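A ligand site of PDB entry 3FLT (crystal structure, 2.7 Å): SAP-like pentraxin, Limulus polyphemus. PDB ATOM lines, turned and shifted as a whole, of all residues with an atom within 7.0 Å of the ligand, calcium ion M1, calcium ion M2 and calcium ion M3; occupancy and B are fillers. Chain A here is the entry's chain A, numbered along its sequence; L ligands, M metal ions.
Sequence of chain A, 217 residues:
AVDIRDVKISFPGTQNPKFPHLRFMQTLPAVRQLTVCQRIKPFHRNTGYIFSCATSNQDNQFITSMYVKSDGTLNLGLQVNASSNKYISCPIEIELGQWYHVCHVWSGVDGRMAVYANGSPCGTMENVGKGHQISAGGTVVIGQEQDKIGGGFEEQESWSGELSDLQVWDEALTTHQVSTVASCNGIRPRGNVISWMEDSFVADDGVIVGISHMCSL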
ATOM      1  N   THR A  47     -20.548 -27.141  12.250  1.00  0.00           N
ATOM      2  CA  THR A  47     -21.117 -25.921  11.698  1.00  0.00           C
ATOM      3  C   THR A  47     -20.294 -25.285  10.608  1.00  0.00           C
ATOM      4  O   THR A  47     -19.069 -25.161  10.717  1.00  0.00           O
ATOM      5  CB  THR A  47     -21.328 -24.871  12.815  1.00  0.00           C
ATOM      6  OG1 THR A  47     -22.355 -25.327  13.708  1.00  0.00           O
ATOM      7  CG2 THR A  47     -21.749 -23.527  12.246  1.00  0.00           C
ATOM      8  N   TYR A  49     -20.752 -22.085   7.375  1.00  0.00           N
ATOM      9  CA  TYR A  49     -21.588 -21.059   6.763  1.00  0.00           C
ATOM     10  C   TYR A  49     -21.563 -21.225   5.260  1.00  0.00           C
ATOM     11  O   TYR A  49     -20.487 -21.280   4.649  1.00  0.00           O
ATOM     12  CB  TYR A  49     -21.117 -19.656   7.164  1.00  0.00           C
ATOM     13  CG  TYR A  49     -21.341 -19.378   8.625  1.00  0.00           C
ATOM     14  CD1 TYR A  49     -20.324 -19.599   9.566  1.00  0.00           C
ATOM     15  CD2 TYR A  49     -22.590 -18.979   9.097  1.00  0.00           C
ATOM     16  CE1 TYR A  49     -20.559 -19.438  10.931  1.00  0.00           C
ATOM     17  CE2 TYR A  49     -22.831 -18.818  10.445  1.00  0.00           C
ATOM     18  CZ  TYR A  49     -21.810 -19.047  11.360  1.00  0.00           C
ATOM     19  OH  TYR A  49     -22.072 -18.919  12.692  1.00  0.00           O
ATOM     20  N   SER A  52     -23.219 -16.164   2.736  1.00  0.00           N
ATOM     21  CA  SER A  52     -22.843 -15.027   3.580  1.00  0.00           C
ATOM     22  C   SER A  52     -23.034 -13.707   2.842  1.00  0.00           C
ATOM     23  O   SER A  52     -22.500 -13.515   1.743  1.00  0.00           O
ATOM     24  CB  SER A  52     -21.378 -15.159   4.001  1.00  0.00           C
ATOM     25  OG  SER A  52     -20.868 -13.949   4.528  1.00  0.00           O
ATOM     26  N   ALA A  54     -22.761  -9.476   3.278  1.00  0.00           N
ATOM     27  CA  ALA A  54     -22.246  -8.382   4.084  1.00  0.00           C
ATOM     28  C   ALA A  54     -22.224  -7.038   3.383  1.00  0.00           C
ATOM     29  O   ALA A  54     -22.059  -6.944   2.174  1.00  0.00           O
ATOM     30  CB  ALA A  54     -20.840  -8.721   4.559  1.00  0.00           C
ATOM     31  N   GLN A  58     -22.382  -3.616   8.093  1.00  0.00           N
ATOM     32  CA  GLN A  58     -22.778  -4.860   8.754  1.00  0.00           C
ATOM     33  C   GLN A  58     -22.297  -6.079   7.975  1.00  0.00           C
ATOM     34  O   GLN A  58     -22.817  -6.382   6.914  1.00  0.00           O
ATOM     35  CB  GLN A  58     -24.307  -4.903   8.883  1.00  0.00           C
ATOM     36  CG  GLN A  58     -24.881  -6.204   9.418  1.00  0.00           C
ATOM     37  CD  GLN A  58     -24.414  -6.523  10.835  1.00  0.00           C
ATOM     38  OE1 GLN A  58     -23.278  -6.969  11.033  1.00  0.00           O
ATOM     39  NE2 GLN A  58     -25.284  -6.288  11.818  1.00  0.00           N
ATOM     40  N   ASP A  59     -21.303  -6.779   8.524  1.00  0.00           N
ATOM     41  CA  ASP A  59     -20.751  -7.961   7.866  1.00  0.00           C
ATOM     42  C   ASP A  59     -21.647  -9.197   8.053  1.00  0.00           C
ATOM     43  O   ASP A  59     -21.489 -10.197   7.352  1.00  0.00           O
ATOM     44  CB  ASP A  59     -19.337  -8.235   8.407  1.00  0.00           C
ATOM     45  CG  ASP A  59     -19.305  -8.463   9.910  1.00  0.00           C
ATOM     46  OD1 ASP A  59     -19.735  -7.561  10.666  1.00  0.00           O
ATOM     47  OD2 ASP A  59     -18.871  -9.555  10.336  1.00  0.00           O
ATOM     48  N   ASN A  60     -22.592  -9.120   8.985  1.00  0.00           N
ATOM     49  CA  ASN A  60     -23.502 -10.220   9.228  1.00  0.00           C
ATOM     50  C   ASN A  60     -24.936  -9.835   8.877  1.00  0.00           C
ATOM     51  O   ASN A  60     -25.835  -9.926   9.714  1.00  0.00           O
ATOM     52  CB  ASN A  60     -23.450 -10.654  10.702  1.00  0.00           C
ATOM     53  CG  ASN A  60     -22.122 -11.293  11.083  1.00  0.00           C
ATOM     54  OD1 ASN A  60     -21.123 -11.136  10.386  1.00  0.00           O
ATOM     55  ND2 ASN A  60     -22.111 -12.016  12.198  1.00  0.00           N
ATOM     56  N   ILE A  63     -26.738 -14.674   6.956  1.00  0.00           N
ATOM     57  CA  ILE A  63     -25.833 -15.818   6.883  1.00  0.00           C
ATOM     58  C   ILE A  63     -26.540 -17.139   7.148  1.00  0.00           C
ATOM     59  O   ILE A  63     -27.151 -17.312   8.191  1.00  0.00           O
ATOM     60  CB  ILE A  63     -24.703 -15.731   7.930  1.00  0.00           C
ATOM     61  CG1 ILE A  63     -24.592 -14.296   8.461  1.00  0.00           C
ATOM     62  CG2 ILE A  63     -23.397 -16.201   7.309  1.00  0.00           C
ATOM     63  CD1 ILE A  63     -23.596 -14.155   9.619  1.00  0.00           C
ATOM     64  N   GLN A  79     -28.911 -16.278  10.437  1.00  0.00           N
ATOM     65  CA  GLN A  79     -28.548 -15.142  11.249  1.00  0.00           C
ATOM     66  C   GLN A  79     -28.837 -13.881  10.452  1.00  0.00           C
ATOM     67  O   GLN A  79     -28.401 -13.761   9.311  1.00  0.00           O
ATOM     68  CB  GLN A  79     -27.062 -15.194  11.637  1.00  0.00           C
ATOM     69  CG  GLN A  79     -26.603 -13.971  12.435  1.00  0.00           C
ATOM     70  CD  GLN A  79     -25.130 -14.024  12.828  1.00  0.00           C
ATOM     71  OE1 GLN A  79     -24.532 -13.006  13.156  1.00  0.00           O
ATOM     72  NE2 GLN A  79     -24.541 -15.222  12.798  1.00  0.00           N
ATOM     73  N   SER A  83     -27.750 -11.137  14.558  1.00  0.00           N
ATOM     74  CA  SER A  83     -28.464 -11.741  15.672  1.00  0.00           C
ATOM     75  C   SER A  83     -27.703 -13.021  15.977  1.00  0.00           C
ATOM     76  O   SER A  83     -26.653 -13.274  15.394  1.00  0.00           O
ATOM     77  CB  SER A  83     -29.911 -12.075  15.279  1.00  0.00           C
ATOM     78  OG  SER A  83     -29.957 -13.110  14.299  1.00  0.00           O
ATOM     79  N   ASN A  85     -27.261 -17.107  15.809  1.00  0.00           N
ATOM     80  CA  ASN A  85     -27.700 -18.088  14.829  1.00  0.00           C
ATOM     81  C   ASN A  85     -28.919 -18.826  15.351  1.00  0.00           C
ATOM     82  O   ASN A  85     -28.883 -19.408  16.432  1.00  0.00           O
ATOM     83  CB  ASN A  85     -26.590 -19.075  14.511  1.00  0.00           C
ATOM     84  CG  ASN A  85     -25.467 -18.442  13.741  1.00  0.00           C
ATOM     85  OD1 ASN A  85     -25.682 -17.875  12.671  1.00  0.00           O
ATOM     86  ND2 ASN A  85     -24.264 -18.529  14.276  1.00  0.00           N
ATOM     87  N   GLU A 145     -17.401 -17.350   5.768  1.00  0.00           N
ATOM     88  CA  GLU A 145     -18.167 -16.329   6.501  1.00  0.00           C
ATOM     89  C   GLU A 145     -17.376 -15.020   6.551  1.00  0.00           C
ATOM     90  O   GLU A 145     -16.301 -14.946   7.146  1.00  0.00           O
ATOM     91  CB  GLU A 145     -18.453 -16.825   7.926  1.00  0.00           C
ATOM     92  CG  GLU A 145     -19.639 -16.184   8.617  1.00  0.00           C
ATOM     93  CD  GLU A 145     -19.403 -14.720   8.991  1.00  0.00           C
ATOM     94  OE1 GLU A 145     -18.389 -14.441   9.668  1.00  0.00           O
ATOM     95  OE2 GLU A 145     -20.233 -13.858   8.619  1.00  0.00           O
ATOM     96  N   GLN A 146     -17.921 -13.978   5.926  1.00  0.00           N
ATOM     97  CA  GLN A 146     -17.249 -12.679   5.869  1.00  0.00           C
ATOM     98  C   GLN A 146     -17.258 -11.898   7.169  1.00  0.00           C
ATOM     99  O   GLN A 146     -18.275 -11.819   7.850  1.00  0.00           O
ATOM    100  CB  GLN A 146     -17.904 -11.795   4.808  1.00  0.00           C
ATOM    101  CG  GLN A 146     -17.971 -12.364   3.421  1.00  0.00           C
ATOM    102  CD  GLN A 146     -18.830 -11.511   2.512  1.00  0.00           C
ATOM    103  OE1 GLN A 146     -18.389 -10.485   1.993  1.00  0.00           O
ATOM    104  NE2 GLN A 146     -20.074 -11.920   2.322  1.00  0.00           N
ATOM    105  N   ASP A 147     -16.119 -11.301   7.497  1.00  0.00           N
ATOM    106  CA  ASP A 147     -16.013 -10.440   8.676  1.00  0.00           C
ATOM    107  C   ASP A 147     -15.661  -9.089   8.090  1.00  0.00           C
ATOM    108  O   ASP A 147     -15.458  -8.112   8.792  1.00  0.00           O
ATOM    109  CB  ASP A 147     -14.920 -10.904   9.623  1.00  0.00           C
ATOM    110  CG  ASP A 147     -15.321 -12.118  10.423  1.00  0.00           C
ATOM    111  OD1 ASP A 147     -16.463 -12.153  10.899  1.00  0.00           O
ATOM    112  OD2 ASP A 147     -14.498 -13.033  10.586  1.00  0.00           O
ATOM    113  N   LYS A 148     -15.608  -9.066   6.769  1.00  0.00           N
ATOM    114  CA  LYS A 148     -15.273  -7.888   5.989  1.00  0.00           C
ATOM    115  C   LYS A 148     -15.750  -8.157   4.555  1.00  0.00           C
ATOM    116  O   LYS A 148     -15.817  -9.315   4.126  1.00  0.00           O
ATOM    117  CB  LYS A 148     -13.766  -7.686   6.014  1.00  0.00           C
ATOM    118  CG  LYS A 148     -13.283  -6.621   5.097  1.00  0.00           C
ATOM    119  CD  LYS A 148     -11.785  -6.495   5.200  1.00  0.00           C
ATOM    120  CE  LYS A 148     -11.089  -7.767   4.807  1.00  0.00           C
ATOM    121  NZ  LYS A 148      -9.622  -7.539   4.698  1.00  0.00           N
ATOM    122  N   GLY A 151     -14.064 -10.851   2.567  1.00  0.00           N
ATOM    123  CA  GLY A 151     -12.928 -11.398   3.276  1.00  0.00           C
ATOM    124  C   GLY A 151     -13.065 -11.567   4.786  1.00  0.00           C
ATOM    125  O   GLY A 151     -14.173 -11.614   5.323  1.00  0.00           O
ATOM    126  N   GLY A 152     -11.913 -11.659   5.454  1.00  0.00           N
ATOM    127  CA  GLY A 152     -11.903 -11.849   6.891  1.00  0.00           C
ATOM    128  C   GLY A 152     -12.478 -13.203   7.232  1.00  0.00           C
ATOM    129  O   GLY A 152     -13.264 -13.328   8.173  1.00  0.00           O
ATOM    130  N   PHE A 153     -12.083 -14.230   6.490  1.00  0.00           N
ATOM    131  CA  PHE A 153     -12.597 -15.571   6.719  1.00  0.00           C
ATOM    132  C   PHE A 153     -11.942 -16.298   7.893  1.00  0.00           C
ATOM    133  O   PHE A 153     -10.771 -16.075   8.181  1.00  0.00           O
ATOM    134  CB  PHE A 153     -12.440 -16.424   5.457  1.00  0.00           C
ATOM    135  CG  PHE A 153     -12.979 -15.768   4.203  1.00  0.00           C
ATOM    136  CD1 PHE A 153     -14.261 -15.201   4.184  1.00  0.00           C
ATOM    137  CD2 PHE A 153     -12.213 -15.741   3.033  1.00  0.00           C
ATOM    138  CE1 PHE A 153     -14.771 -14.632   3.010  1.00  0.00           C
ATOM    139  CE2 PHE A 153     -12.723 -15.172   1.860  1.00  0.00           C
ATOM    140  CZ  PHE A 153     -14.001 -14.613   1.851  1.00  0.00           C
ATOM    141  N   GLU A 154     -12.718 -17.144   8.551  1.00  0.00           N
ATOM    142  CA  GLU A 154     -12.251 -17.948   9.684  1.00  0.00           C
ATOM    143  C   GLU A 154     -12.430 -19.417   9.300  1.00  0.00           C
ATOM    144  O   GLU A 154     -13.507 -19.810   8.867  1.00  0.00           O
ATOM    145  CB  GLU A 154     -13.070 -17.623  10.934  1.00  0.00           C
ATOM    146  CG  GLU A 154     -13.220 -16.139  11.191  1.00  0.00           C
ATOM    147  CD  GLU A 154     -13.592 -15.825  12.632  1.00  0.00           C
ATOM    148  OE1 GLU A 154     -12.813 -16.211  13.533  1.00  0.00           O
ATOM    149  OE2 GLU A 154     -14.653 -15.218  12.878  1.00  0.00           O
ATOM    150  N   GLN A 156     -12.740 -22.218  11.066  1.00  0.00           N
ATOM    151  CA  GLN A 156     -13.755 -22.977  11.784  1.00  0.00           C
ATOM    152  C   GLN A 156     -15.167 -22.571  11.431  1.00  0.00           C
ATOM    153  O   GLN A 156     -16.124 -23.151  11.939  1.00  0.00           O
ATOM    154  CB  GLN A 156     -13.531 -22.928  13.303  1.00  0.00           C
ATOM    155  CG  GLN A 156     -14.017 -21.701  14.072  1.00  0.00           C
ATOM    156  CD  GLN A 156     -13.320 -20.406  13.686  1.00  0.00           C
ATOM    157  OE1 GLN A 156     -12.170 -20.409  13.245  1.00  0.00           O
ATOM    158  NE2 GLN A 156     -14.021 -19.294  13.862  1.00  0.00           N
ATOM    159  N   GLU A 157     -15.295 -21.572  10.547  1.00  0.00           N
ATOM    160  CA  GLU A 157     -16.618 -21.112  10.119  1.00  0.00           C
ATOM    161  C   GLU A 157     -16.874 -21.392   8.644  1.00  0.00           C
ATOM    162  O   GLU A 157     -17.928 -21.059   8.111  1.00  0.00           O
ATOM    163  CB  GLU A 157     -16.773 -19.608  10.385  1.00  0.00           C
ATOM    164  CG  GLU A 157     -16.496 -19.203  11.815  1.00  0.00           C
ATOM    165  CD  GLU A 157     -16.944 -17.794  12.138  1.00  0.00           C
ATOM    166  OE1 GLU A 157     -16.539 -16.839  11.447  1.00  0.00           O
ATOM    167  OE2 GLU A 157     -17.726 -17.629  13.104  1.00  0.00           O
HETATM  168  C1  LIG L   1     -20.090 -14.934  13.236  1.00  0.00           C
HETATM  169  C2  LIG L   1     -21.211 -15.784  13.873  1.00  0.00           C
HETATM  170  O1  LIG L   1     -17.268 -14.138  12.935  1.00  0.00           O
HETATM  171  O2  LIG L   1     -19.026 -12.452  12.282  1.00  0.00           O
HETATM  172  O3  LIG L   1     -17.791 -12.037  14.423  1.00  0.00           O
HETATM  173  O4  LIG L   1     -19.567 -13.982  14.193  1.00  0.00           O
HETATM  174  N1  LIG L   1     -20.725 -17.187  14.052  1.00  0.00           N
HETATM  175  P1  LIG L   1     -18.426 -13.140  13.436  1.00  0.00           P
HETATM  176 CA    CA M   1     -18.971 -12.069   9.852  1.00  0.00          CA
HETATM  177 CA    CA M   2     -16.382 -14.642  10.877  1.00  0.00          CA
HETATM  178 CA    CA M   3     -16.036 -15.538  14.706  1.00  0.00          CA
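Of the 21 residues printed, 5 come within 4 Å of calcium ion M1. The nearest printed residue that does not touch calcium ion M1 is Ile 63 (5.1 Å).
Residues that only touch the ligand: Gln 79 (3.5 Å) and Asn 85 (3.8 Å). Hydrophobic or aromatic side chains within 4 Å of the ligand: Tyr 49. Of the 21 residues printed, 9 come within 4 Å of the ligand.
Calcium ion M3 is bound by the side-chain carboxylate (OE2) of Glu 154 (2.3 Å) and an oxygen (O1) of the ligand (2.6 Å). Calcium ion M3 has two donor atoms within binding distance. Slightly farther from calcium ion M3 lies OE2 of Glu 157 (3.1 Å).
Of the 21 residues printed, 4 come within 4 Å of calcium ion M2.
Calcium ion M1 is bound by O of Gln 146 (2.1 Å), OD1 of Asn 60 (2.4 Å), OE1 of Glu 145 (2.4 Å), O2 of the ligand (2.5 Å), OE2 of Glu 145 (2.5 Å), OD2 of Asp 59 (2.6 Å) and OD1 of Asp 147 (2.7 Å). Calcium ion M1 has seven donor atoms within binding distance.
Two residues have an atom within 4 Å of calcium ion M3: Glu 154 and Glu 157.
The side-chain amide nitrogen of Gln 146 sits at hydrogen-bond distance from the backbone carbonyl oxygen of Ser 52. O of Glu 157 is in hydrogen-bond range of N of Tyr 49, at 3.1 Å. ND2 of Asn 60 sits at hydrogen-bond distance from OE1 of Gln 79. The side-chain amide oxygen of Gln 58 sits at hydrogen-bond distance from the backbone NH of Asn 60, 3.0 Å away. OH of Tyr 49 sits at hydrogen-bond distance from ND2 of Asn 85 (2.7 Å). The side-chain amide nitrogen (NE2) of Gln 79 lies within hydrogen-bond range of the side-chain amide oxygen (OD1) of Asn 85 (2.9 Å). The backbone NH of Ile 63 sits at hydrogen-bond distance from the backbone carbonyl oxygen of Gln 79. The side-chain amide oxygen (OE1) of Gln 79 sits close to the backbone carbonyl oxygen (O) of Ser 83 (3.1 Å).
Calcium ion M2 is bound by the side-chain carboxylate (OE1) of Glu 157, an oxygen (O1) of the ligand, the side-chain carboxylate (OE1) of Glu 145, the side-chain carboxylate (OD1) of Asp 147, the side-chain carboxylate (OD2) of Asp 147 and the side-chain carboxylate (OE2) of Glu 154.
The side-chain hydroxyl (OH) of Tyr 49 is in hydrogen-bond range of a nitrogen (N1) of the ligand (2.6 Å).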
